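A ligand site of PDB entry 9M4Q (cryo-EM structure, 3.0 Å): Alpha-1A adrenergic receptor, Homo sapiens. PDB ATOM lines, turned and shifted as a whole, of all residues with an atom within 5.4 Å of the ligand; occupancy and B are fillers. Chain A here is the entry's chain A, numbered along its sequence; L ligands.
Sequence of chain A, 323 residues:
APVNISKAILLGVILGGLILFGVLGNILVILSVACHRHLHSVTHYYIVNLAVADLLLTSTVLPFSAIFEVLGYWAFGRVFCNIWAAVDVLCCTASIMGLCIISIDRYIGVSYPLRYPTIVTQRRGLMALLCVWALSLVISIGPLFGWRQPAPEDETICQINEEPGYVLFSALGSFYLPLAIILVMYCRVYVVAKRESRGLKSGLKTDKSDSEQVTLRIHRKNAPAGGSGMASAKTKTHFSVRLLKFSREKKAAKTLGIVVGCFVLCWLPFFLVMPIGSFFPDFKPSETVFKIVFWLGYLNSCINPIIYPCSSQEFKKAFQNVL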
ATOM      1  N   VAL A  61      16.340  19.741 -30.872  1.00  0.00           N
ATOM      2  CA  VAL A  61      16.958  20.299 -29.667  1.00  0.00           C
ATOM      3  C   VAL A  61      15.889  20.752 -28.683  1.00  0.00           C
ATOM      4  O   VAL A  61      16.027  20.550 -27.459  1.00  0.00           O
ATOM      5  CB  VAL A  61      17.918  21.434 -30.044  1.00  0.00           C
ATOM      6  CG1 VAL A  61      17.184  22.582 -30.660  1.00  0.00           C
ATOM      7  CG2 VAL A  61      18.694  21.915 -28.832  1.00  0.00           C
ATOM      8  N   SER A  65      15.455  19.551 -24.788  1.00  0.00           N
ATOM      9  CA  SER A  65      15.527  20.489 -23.663  1.00  0.00           C
ATOM     10  C   SER A  65      14.281  20.379 -22.795  1.00  0.00           C
ATOM     11  O   SER A  65      14.369  20.423 -21.566  1.00  0.00           O
ATOM     12  CB  SER A  65      15.700  21.913 -24.188  1.00  0.00           C
ATOM     13  OG  SER A  65      16.117  22.782 -23.144  1.00  0.00           O
ATOM     14  N   PHE A  68      14.531  17.252 -20.733  1.00  0.00           N
ATOM     15  CA  PHE A  68      15.493  17.471 -19.661  1.00  0.00           C
ATOM     16  C   PHE A  68      14.869  18.284 -18.541  1.00  0.00           C
ATOM     17  O   PHE A  68      15.046  17.983 -17.353  1.00  0.00           O
ATOM     18  CB  PHE A  68      16.733  18.187 -20.203  1.00  0.00           C
ATOM     19  CG  PHE A  68      17.789  18.440 -19.159  1.00  0.00           C
ATOM     20  CD1 PHE A  68      17.747  19.589 -18.387  1.00  0.00           C
ATOM     21  CD2 PHE A  68      18.829  17.545 -18.970  1.00  0.00           C
ATOM     22  CE1 PHE A  68      18.715  19.822 -17.425  1.00  0.00           C
ATOM     23  CE2 PHE A  68      19.797  17.784 -18.021  1.00  0.00           C
ATOM     24  CZ  PHE A  68      19.737  18.919 -17.246  1.00  0.00           C
ATOM     25  N   CYS A  81      24.026  13.667 -25.670  1.00  0.00           N
ATOM     26  CA  CYS A  81      24.202  15.000 -25.104  1.00  0.00           C
ATOM     27  C   CYS A  81      25.099  15.860 -25.987  1.00  0.00           C
ATOM     28  O   CYS A  81      24.794  17.041 -26.244  1.00  0.00           O
ATOM     29  CB  CYS A  81      24.779  14.902 -23.691  1.00  0.00           C
ATOM     30  SG  CYS A  81      25.419  16.461 -23.031  1.00  0.00           S
ATOM     31  N   TRP A  84      23.296  16.782 -29.072  1.00  0.00           N
ATOM     32  CA  TRP A  84      22.268  17.763 -28.749  1.00  0.00           C
ATOM     33  C   TRP A  84      22.863  19.163 -28.684  1.00  0.00           C
ATOM     34  O   TRP A  84      22.345  20.103 -29.289  1.00  0.00           O
ATOM     35  CB  TRP A  84      21.626  17.383 -27.418  1.00  0.00           C
ATOM     36  CG  TRP A  84      20.584  18.323 -26.912  1.00  0.00           C
ATOM     37  CD1 TRP A  84      19.587  18.893 -27.625  1.00  0.00           C
ATOM     38  CD2 TRP A  84      20.429  18.765 -25.559  1.00  0.00           C
ATOM     39  NE1 TRP A  84      18.816  19.682 -26.809  1.00  0.00           N
ATOM     40  CE2 TRP A  84      19.307  19.627 -25.536  1.00  0.00           C
ATOM     41  CE3 TRP A  84      21.119  18.534 -24.368  1.00  0.00           C
ATOM     42  CZ2 TRP A  84      18.872  20.251 -24.372  1.00  0.00           C
ATOM     43  CZ3 TRP A  84      20.683  19.149 -23.215  1.00  0.00           C
ATOM     44  CH2 TRP A  84      19.569  19.992 -23.224  1.00  0.00           C
ATOM     45  N   ALA A  85      23.980  19.309 -27.965  1.00  0.00           N
ATOM     46  CA  ALA A  85      24.640  20.607 -27.892  1.00  0.00           C
ATOM     47  C   ALA A  85      25.109  21.060 -29.270  1.00  0.00           C
ATOM     48  O   ALA A  85      24.948  22.234 -29.643  1.00  0.00           O
ATOM     49  CB  ALA A  85      25.829  20.537 -26.929  1.00  0.00           C
ATOM     50  N   ASP A  88      22.146  22.202 -31.327  1.00  0.00           N
ATOM     51  CA  ASP A  88      21.695  23.499 -30.830  1.00  0.00           C
ATOM     52  C   ASP A  88      22.562  24.615 -31.388  1.00  0.00           C
ATOM     53  O   ASP A  88      22.055  25.595 -31.953  1.00  0.00           O
ATOM     54  CB  ASP A  88      21.729  23.504 -29.308  1.00  0.00           C
ATOM     55  CG  ASP A  88      21.156  24.782 -28.722  1.00  0.00           C
ATOM     56  OD1 ASP A  88      20.486  25.526 -29.458  1.00  0.00           O
ATOM     57  OD2 ASP A  88      21.399  25.043 -27.522  1.00  0.00           O
ATOM     58  N   VAL A  89      23.880  24.494 -31.235  1.00  0.00           N
ATOM     59  CA  VAL A  89      24.782  25.534 -31.711  1.00  0.00           C
ATOM     60  C   VAL A  89      24.676  25.668 -33.226  1.00  0.00           C
ATOM     61  O   VAL A  89      24.651  26.778 -33.769  1.00  0.00           O
ATOM     62  CB  VAL A  89      26.224  25.251 -31.270  1.00  0.00           C
ATOM     63  CG1 VAL A  89      27.159  26.316 -31.814  1.00  0.00           C
ATOM     64  CG2 VAL A  89      26.307  25.202 -29.757  1.00  0.00           C
ATOM     65  N   CYS A  92      21.285  27.482 -34.130  1.00  0.00           N
ATOM     66  CA  CYS A  92      21.283  28.880 -33.683  1.00  0.00           C
ATOM     67  C   CYS A  92      22.390  29.709 -34.333  1.00  0.00           C
ATOM     68  O   CYS A  92      22.315  30.940 -34.278  1.00  0.00           O
ATOM     69  CB  CYS A  92      21.425  28.944 -32.163  1.00  0.00           C
ATOM     70  SG  CYS A  92      21.451  30.624 -31.506  1.00  0.00           S
ATOM     71  N   THR A  93      23.379  29.073 -34.939  1.00  0.00           N
ATOM     72  CA  THR A  93      24.441  29.783 -35.646  1.00  0.00           C
ATOM     73  C   THR A  93      24.252  29.787 -37.159  1.00  0.00           C
ATOM     74  O   THR A  93      24.826  30.645 -37.830  1.00  0.00           O
ATOM     75  CB  THR A  93      25.805  29.155 -35.317  1.00  0.00           C
ATOM     76  OG1 THR A  93      25.947  29.021 -33.896  1.00  0.00           O
ATOM     77  CG2 THR A  93      26.939  30.021 -35.837  1.00  0.00           C
ATOM     78  N   LEU A 144      33.551  23.279 -30.556  1.00  0.00           N
ATOM     79  CA  LEU A 144      33.025  22.186 -29.747  1.00  0.00           C
ATOM     80  C   LEU A 144      33.778  20.883 -30.012  1.00  0.00           C
ATOM     81  O   LEU A 144      34.422  20.331 -29.117  1.00  0.00           O
ATOM     82  CB  LEU A 144      31.533  22.006 -30.029  1.00  0.00           C
ATOM     83  CG  LEU A 144      30.595  23.066 -29.438  1.00  0.00           C
ATOM     84  CD1 LEU A 144      29.197  22.904 -29.992  1.00  0.00           C
ATOM     85  CD2 LEU A 144      30.576  22.960 -27.914  1.00  0.00           C
ATOM     86  N   CYS A 158      24.664  16.864 -18.422  1.00  0.00           N
ATOM     87  CA  CYS A 158      24.772  17.454 -19.751  1.00  0.00           C
ATOM     88  C   CYS A 158      24.808  18.968 -19.564  1.00  0.00           C
ATOM     89  O   CYS A 158      23.766  19.623 -19.563  1.00  0.00           O
ATOM     90  CB  CYS A 158      23.612  17.011 -20.641  1.00  0.00           C
ATOM     91  SG  CYS A 158      23.775  17.468 -22.390  1.00  0.00           S
ATOM     92  N   GLN A 159      26.011  19.515 -19.415  1.00  0.00           N
ATOM     93  CA  GLN A 159      26.226  20.919 -19.120  1.00  0.00           C
ATOM     94  C   GLN A 159      26.801  21.638 -20.335  1.00  0.00           C
ATOM     95  O   GLN A 159      27.017  21.044 -21.402  1.00  0.00           O
ATOM     96  CB  GLN A 159      27.148  21.086 -17.908  1.00  0.00           C
ATOM     97  CG  GLN A 159      26.405  21.315 -16.600  1.00  0.00           C
ATOM     98  CD  GLN A 159      27.329  21.337 -15.403  1.00  0.00           C
ATOM     99  OE1 GLN A 159      28.546  21.163 -15.537  1.00  0.00           O
ATOM    100  NE2 GLN A 159      26.769  21.535 -14.215  1.00  0.00           N
ATOM    101  N   ILE A 160      27.055  22.932 -20.165  1.00  0.00           N
ATOM    102  CA  ILE A 160      27.583  23.788 -21.213  1.00  0.00           C
ATOM    103  C   ILE A 160      29.011  24.196 -20.847  1.00  0.00           C
ATOM    104  O   ILE A 160      29.295  24.501 -19.683  1.00  0.00           O
ATOM    105  CB  ILE A 160      26.693  25.023 -21.425  1.00  0.00           C
ATOM    106  CG1 ILE A 160      27.340  25.987 -22.424  1.00  0.00           C
ATOM    107  CG2 ILE A 160      26.429  25.738 -20.098  1.00  0.00           C
ATOM    108  CD1 ILE A 160      26.382  27.008 -23.001  1.00  0.00           C
ATOM    109  N   ASN A 161      29.890  24.200 -21.846  1.00  0.00           N
ATOM    110  CA  ASN A 161      31.289  24.548 -21.620  1.00  0.00           C
ATOM    111  C   ASN A 161      31.408  25.934 -20.998  1.00  0.00           C
ATOM    112  O   ASN A 161      31.076  26.938 -21.644  1.00  0.00           O
ATOM    113  CB  ASN A 161      32.071  24.503 -22.936  1.00  0.00           C
ATOM    114  CG  ASN A 161      32.253  23.088 -23.450  1.00  0.00           C
ATOM    115  OD1 ASN A 161      32.532  22.165 -22.691  1.00  0.00           O
ATOM    116  ND2 ASN A 161      32.090  22.916 -24.762  1.00  0.00           N
ATOM    117  N   TYR A 166      36.257  28.986 -24.810  1.00  0.00           N
ATOM    118  CA  TYR A 166      35.221  28.534 -25.724  1.00  0.00           C
ATOM    119  C   TYR A 166      34.080  29.527 -25.853  1.00  0.00           C
ATOM    120  O   TYR A 166      33.585  29.752 -26.969  1.00  0.00           O
ATOM    121  CB  TYR A 166      34.648  27.184 -25.268  1.00  0.00           C
ATOM    122  CG  TYR A 166      33.358  26.833 -25.984  1.00  0.00           C
ATOM    123  CD1 TYR A 166      33.374  26.287 -27.253  1.00  0.00           C
ATOM    124  CD2 TYR A 166      32.127  27.073 -25.391  1.00  0.00           C
ATOM    125  CE1 TYR A 166      32.200  25.973 -27.911  1.00  0.00           C
ATOM    126  CE2 TYR A 166      30.954  26.768 -26.038  1.00  0.00           C
ATOM    127  CZ  TYR A 166      30.992  26.207 -27.299  1.00  0.00           C
ATOM    128  OH  TYR A 166      29.830  25.900 -27.955  1.00  0.00           O
ATOM    129  N   VAL A 167      33.634  30.103 -24.739  1.00  0.00           N
ATOM    130  CA  VAL A 167      32.487  31.006 -24.791  1.00  0.00           C
ATOM    131  C   VAL A 167      32.823  32.235 -25.612  1.00  0.00           C
ATOM    132  O   VAL A 167      32.003  32.724 -26.396  1.00  0.00           O
ATOM    133  CB  VAL A 167      32.019  31.378 -23.371  1.00  0.00           C
ATOM    134  CG1 VAL A 167      31.751  30.126 -22.539  1.00  0.00           C
ATOM    135  CG2 VAL A 167      33.029  32.279 -22.696  1.00  0.00           C
ATOM    136  N   SER A 170      32.819  31.246 -29.319  1.00  0.00           N
ATOM    137  CA  SER A 170      31.475  30.920 -29.799  1.00  0.00           C
ATOM    138  C   SER A 170      30.620  32.179 -29.926  1.00  0.00           C
ATOM    139  O   SER A 170      29.949  32.373 -30.948  1.00  0.00           O
ATOM    140  CB  SER A 170      30.810  29.921 -28.861  1.00  0.00           C
ATOM    141  OG  SER A 170      29.500  29.621 -29.293  1.00  0.00           O
ATOM    142  N   ALA A 171      30.653  33.053 -28.919  1.00  0.00           N
ATOM    143  CA  ALA A 171      29.863  34.280 -28.992  1.00  0.00           C
ATOM    144  C   ALA A 171      30.348  35.170 -30.124  1.00  0.00           C
ATOM    145  O   ALA A 171      29.531  35.760 -30.843  1.00  0.00           O
ATOM    146  CB  ALA A 171      29.944  35.023 -27.651  1.00  0.00           C
ATOM    147  N   SER A 174      29.520  33.309 -33.640  1.00  0.00           N
ATOM    148  CA  SER A 174      28.147  32.872 -33.829  1.00  0.00           C
ATOM    149  C   SER A 174      27.131  34.001 -33.735  1.00  0.00           C
ATOM    150  O   SER A 174      26.153  33.996 -34.477  1.00  0.00           O
ATOM    151  CB  SER A 174      27.791  31.791 -32.798  1.00  0.00           C
ATOM    152  OG  SER A 174      26.517  31.239 -33.070  1.00  0.00           O
ATOM    153  N   TRP A 267      17.663  36.368 -28.778  1.00  0.00           N
ATOM    154  CA  TRP A 267      18.936  35.701 -28.500  1.00  0.00           C
ATOM    155  C   TRP A 267      19.963  36.602 -27.826  1.00  0.00           C
ATOM    156  O   TRP A 267      21.030  36.100 -27.448  1.00  0.00           O
ATOM    157  CB  TRP A 267      19.528  35.139 -29.798  1.00  0.00           C
ATOM    158  CG  TRP A 267      19.058  33.746 -30.094  1.00  0.00           C
ATOM    159  CD1 TRP A 267      18.373  33.340 -31.194  1.00  0.00           C
ATOM    160  CD2 TRP A 267      19.236  32.586 -29.270  1.00  0.00           C
ATOM    161  NE1 TRP A 267      18.114  31.993 -31.109  1.00  0.00           N
ATOM    162  CE2 TRP A 267      18.639  31.509 -29.943  1.00  0.00           C
ATOM    163  CE3 TRP A 267      19.854  32.364 -28.035  1.00  0.00           C
ATOM    164  CZ2 TRP A 267      18.635  30.220 -29.413  1.00  0.00           C
ATOM    165  CZ3 TRP A 267      19.845  31.089 -27.515  1.00  0.00           C
ATOM    166  CH2 TRP A 267      19.236  30.024 -28.205  1.00  0.00           C
ATOM    167  N   PHE A 270      21.000  35.660 -23.884  1.00  0.00           N
ATOM    168  CA  PHE A 270      21.889  34.517 -23.679  1.00  0.00           C
ATOM    169  C   PHE A 270      23.340  34.890 -23.974  1.00  0.00           C
ATOM    170  O   PHE A 270      24.240  34.591 -23.181  1.00  0.00           O
ATOM    171  CB  PHE A 270      21.443  33.349 -24.557  1.00  0.00           C
ATOM    172  CG  PHE A 270      22.444  32.243 -24.640  1.00  0.00           C
ATOM    173  CD1 PHE A 270      23.107  31.805 -23.513  1.00  0.00           C
ATOM    174  CD2 PHE A 270      22.708  31.629 -25.847  1.00  0.00           C
ATOM    175  CE1 PHE A 270      24.032  30.789 -23.594  1.00  0.00           C
ATOM    176  CE2 PHE A 270      23.633  30.612 -25.928  1.00  0.00           C
ATOM    177  CZ  PHE A 270      24.297  30.188 -24.803  1.00  0.00           C
ATOM    178  N   PHE A 271      23.583  35.526 -25.120  1.00  0.00           N
ATOM    179  CA  PHE A 271      24.937  35.908 -25.492  1.00  0.00           C
ATOM    180  C   PHE A 271      25.451  37.093 -24.671  1.00  0.00           C
ATOM    181  O   PHE A 271      26.638  37.410 -24.772  1.00  0.00           O
ATOM    182  CB  PHE A 271      24.999  36.245 -26.981  1.00  0.00           C
ATOM    183  CG  PHE A 271      24.852  35.034 -27.865  1.00  0.00           C
ATOM    184  CD1 PHE A 271      25.867  34.117 -27.976  1.00  0.00           C
ATOM    185  CD2 PHE A 271      23.685  34.833 -28.591  1.00  0.00           C
ATOM    186  CE1 PHE A 271      25.735  33.014 -28.792  1.00  0.00           C
ATOM    187  CE2 PHE A 271      23.553  33.730 -29.407  1.00  0.00           C
ATOM    188  CZ  PHE A 271      24.581  32.814 -29.502  1.00  0.00           C
ATOM    189  N   MET A 274      26.129  34.793 -20.937  1.00  0.00           N
ATOM    190  CA  MET A 274      27.150  33.748 -20.926  1.00  0.00           C
ATOM    191  C   MET A 274      28.552  34.356 -20.905  1.00  0.00           C
ATOM    192  O   MET A 274      29.336  34.028 -19.989  1.00  0.00           O
ATOM    193  CB  MET A 274      26.935  32.789 -22.100  1.00  0.00           C
ATOM    194  CG  MET A 274      28.060  31.774 -22.318  1.00  0.00           C
ATOM    195  SD  MET A 274      28.018  30.973 -23.932  1.00  0.00           S
ATOM    196  CE  MET A 274      27.994  32.384 -25.031  1.00  0.00           C
ATOM    197  N   PHE A 290      19.249  31.479 -16.277  1.00  0.00           N
ATOM    198  CA  PHE A 290      19.992  30.944 -17.415  1.00  0.00           C
ATOM    199  C   PHE A 290      19.070  30.091 -18.296  1.00  0.00           C
ATOM    200  O   PHE A 290      19.050  30.235 -19.533  1.00  0.00           O
ATOM    201  CB  PHE A 290      21.177  30.162 -16.838  1.00  0.00           C
ATOM    202  CG  PHE A 290      22.186  29.675 -17.834  1.00  0.00           C
ATOM    203  CD1 PHE A 290      22.992  30.570 -18.530  1.00  0.00           C
ATOM    204  CD2 PHE A 290      22.458  28.321 -17.950  1.00  0.00           C
ATOM    205  CE1 PHE A 290      23.963  30.121 -19.409  1.00  0.00           C
ATOM    206  CE2 PHE A 290      23.447  27.866 -18.817  1.00  0.00           C
ATOM    207  CZ  PHE A 290      24.200  28.766 -19.547  1.00  0.00           C
ATOM    208  N   LYS A 291      18.241  29.269 -17.653  1.00  0.00           N
ATOM    209  CA  LYS A 291      17.236  28.505 -18.370  1.00  0.00           C
ATOM    210  C   LYS A 291      16.225  29.428 -19.063  1.00  0.00           C
ATOM    211  O   LYS A 291      15.824  29.174 -20.201  1.00  0.00           O
ATOM    212  CB  LYS A 291      16.520  27.570 -17.395  1.00  0.00           C
ATOM    213  CG  LYS A 291      17.476  26.649 -16.645  1.00  0.00           C
ATOM    214  CD  LYS A 291      16.776  25.872 -15.542  1.00  0.00           C
ATOM    215  CE  LYS A 291      16.252  24.538 -16.019  1.00  0.00           C
ATOM    216  NZ  LYS A 291      17.114  23.404 -15.586  1.00  0.00           N
ATOM    217  N   PHE A 294      17.778  30.849 -22.261  1.00  0.00           N
ATOM    218  CA  PHE A 294      17.718  29.860 -23.338  1.00  0.00           C
ATOM    219  C   PHE A 294      16.310  29.733 -23.901  1.00  0.00           C
ATOM    220  O   PHE A 294      16.123  29.673 -25.126  1.00  0.00           O
ATOM    221  CB  PHE A 294      18.221  28.495 -22.891  1.00  0.00           C
ATOM    222  CG  PHE A 294      19.693  28.432 -22.726  1.00  0.00           C
ATOM    223  CD1 PHE A 294      20.509  28.243 -23.812  1.00  0.00           C
ATOM    224  CD2 PHE A 294      20.256  28.578 -21.478  1.00  0.00           C
ATOM    225  CE1 PHE A 294      21.876  28.183 -23.665  1.00  0.00           C
ATOM    226  CE2 PHE A 294      21.601  28.527 -21.327  1.00  0.00           C
ATOM    227  CZ  PHE A 294      22.422  28.330 -22.417  1.00  0.00           C
ATOM    228  N   TYR A 298      14.979  30.323 -27.690  1.00  0.00           N
ATOM    229  CA  TYR A 298      14.258  29.330 -28.476  1.00  0.00           C
ATOM    230  C   TYR A 298      12.921  29.867 -28.959  1.00  0.00           C
ATOM    231  O   TYR A 298      12.429  29.456 -30.022  1.00  0.00           O
ATOM    232  CB  TYR A 298      14.035  28.052 -27.664  1.00  0.00           C
ATOM    233  CG  TYR A 298      15.296  27.303 -27.306  1.00  0.00           C
ATOM    234  CD1 TYR A 298      16.138  26.813 -28.283  1.00  0.00           C
ATOM    235  CD2 TYR A 298      15.617  27.049 -25.981  1.00  0.00           C
ATOM    236  CE1 TYR A 298      17.289  26.108 -27.955  1.00  0.00           C
ATOM    237  CE2 TYR A 298      16.752  26.354 -25.641  1.00  0.00           C
ATOM    238  CZ  TYR A 298      17.588  25.876 -26.628  1.00  0.00           C
ATOM    239  OH  TYR A 298      18.717  25.181 -26.296  1.00  0.00           O
HETATM  240  N1  LIG L   1      23.864  25.354 -26.298  1.00  0.00           N
HETATM  241  C1  LIG L   1      23.385  21.659 -23.128  1.00  0.00           C
HETATM  242  C2  LIG L   1      21.441  22.647 -23.882  1.00  0.00           C
HETATM  243  C3  LIG L   1      21.079  24.159 -21.138  1.00  0.00           C
HETATM  244  C4  LIG L   1      21.710  25.410 -20.546  1.00  0.00           C
HETATM  245  C5  LIG L   1      21.678  24.326 -18.461  1.00  0.00           C
HETATM  246  C6  LIG L   1      21.372  23.523 -16.178  1.00  0.00           C
HETATM  247  C7  LIG L   1      19.908  22.753 -17.956  1.00  0.00           C
HETATM  248  C8  LIG L   1      27.327  30.363 -27.554  1.00  0.00           C
HETATM  249  C9  LIG L   1      26.194  28.369 -27.942  1.00  0.00           C
HETATM  250  C10 LIG L   1      24.816  28.380 -28.140  1.00  0.00           C
HETATM  251  C11 LIG L   1      24.029  27.373 -27.592  1.00  0.00           C
HETATM  252  C12 LIG L   1      24.644  26.335 -26.825  1.00  0.00           C
HETATM  253  C13 LIG L   1      25.977  26.333 -26.630  1.00  0.00           C
HETATM  254  C14 LIG L   1      26.787  27.360 -27.185  1.00  0.00           C
HETATM  255  C15 LIG L   1      26.527  25.277 -25.860  1.00  0.00           C
HETATM  256  C16 LIG L   1      24.416  24.370 -25.575  1.00  0.00           C
HETATM  257  C17 LIG L   1      24.038  22.046 -24.455  1.00  0.00           C
HETATM  258  C18 LIG L   1      22.065  23.508 -24.970  1.00  0.00           C
HETATM  259  C19 LIG L   1      22.233  23.189 -21.499  1.00  0.00           C
HETATM  260  C20 LIG L   1      22.066  24.316 -17.097  1.00  0.00           C
HETATM  261  C21 LIG L   1      20.289  22.734 -16.610  1.00  0.00           C
HETATM  262  C22 LIG L   1      20.608  23.558 -18.893  1.00  0.00           C
HETATM  263  C23 LIG L   1      24.453  29.285 -30.263  1.00  0.00           C
HETATM  264  N2  LIG L   1      25.736  24.337 -25.354  1.00  0.00           N
HETATM  265  N3  LIG L   1      23.548  23.346 -25.024  1.00  0.00           N
HETATM  266  N4  LIG L   1      22.328  22.528 -22.797  1.00  0.00           N
HETATM  267  N5  LIG L   1      27.958  25.233 -25.625  1.00  0.00           N
HETATM  268  O1  LIG L   1      26.987  29.377 -28.481  1.00  0.00           O
HETATM  269  O2  LIG L   1      23.070  22.981 -20.689  1.00  0.00           O
HETATM  270  O3  LIG L   1      22.409  25.154 -19.374  1.00  0.00           O
HETATM  271  O4  LIG L   1      20.189  23.534 -20.255  1.00  0.00           O
HETATM  272  O5  LIG L   1      24.224  29.398 -28.885  1.00  0.00           O
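OG of Ser 170 is in hydrogen-bond range of O1 of the ligand, 2.7 Å away. The side-chain carboxylate (OD2) of Asp 88 is in hydrogen-bond range of a nitrogen (N1) of the ligand, at 2.8 Å. A nitrogen (N5) of the ligand sits at hydrogen-bond distance from the side-chain hydroxyl of Tyr 166 (3.1 Å).
CE1 of Phe 68 touches C7 of the ligand, at 3.2 Å. CH2 of Trp 84 touches C2 of the ligand, 3.3 Å away. Ala 85 touches the ligand (CB to C17, 3.4 Å). Val 89 touches the ligand (CG2 to C13, 3.3 Å). SG of Cys 92 touches C23 of the ligand, 3.5 Å away. OG1 of Thr 93 touches C23 of the ligand (3.9 Å). Cys 158 touches the ligand. Gln 159 touches the ligand. CD1 of Ile 160 touches C15 of the ligand, 3.3 Å away. Ser 174 touches the ligand (OG to C23, 3.99 Å). Phe 270 touches the ligand (CE2 to O5, 3.3 Å). Phe 271 touches the ligand (CE1 to C8, 3.3 Å). Met 274 touches the ligand. CE2 of Phe 290 touches O3 of the ligand, 3.0 Å away. NZ of Lys 291 touches C21 of the ligand, 3.4 Å away. CE2 of Phe 294 touches C4 of the ligand, at 3.2 Å. Tyr 298 touches the ligand. Hydrophobic or aromatic side chains within 4 Å of the ligand: Phe 68, Trp 84, Ala 85, Val 89, Ile 160, Tyr 166, Phe 270, Phe 271, Met 274, Phe 290 and Phe 294. 20 residues have an atom within 4 Å of the ligand: Phe 68, Trp 84, Ala 85, Asp 88, Val 89, Cys 92, Thr 93, Cys 158, Gln 159, Ile 160, Tyr 166, Ser 170, Ser 174, Phe 270, Phe 271, Met 274, Phe 290, Lys 291, Phe 294 and Tyr 298.
OD2 of Asp 88 is in hydrogen-bond range of OH of Tyr 298, at 3.0 Å. The backbone carbonyl oxygen of Val 61 sits at hydrogen-bond distance from the indole nitrogen of Trp 84, 3.0 Å away. The side-chain hydroxyl (OG1) of Thr 93 lies within hydrogen-bond range of the backbone carbonyl oxygen (O) of Val 89 (2.6 Å). The side-chain sulfur (SG) of Cys 92 sits close to the indole nitrogen (NE1) of Trp 267. SG of Cys 81 is disulfide-bonded to SG of Cys 158, at 2.0 Å. The side-chain hydroxyl (OG) of Ser 174 is in hydrogen-bond range of the side-chain hydroxyl (OG1) of Thr 93, at 2.4 Å.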
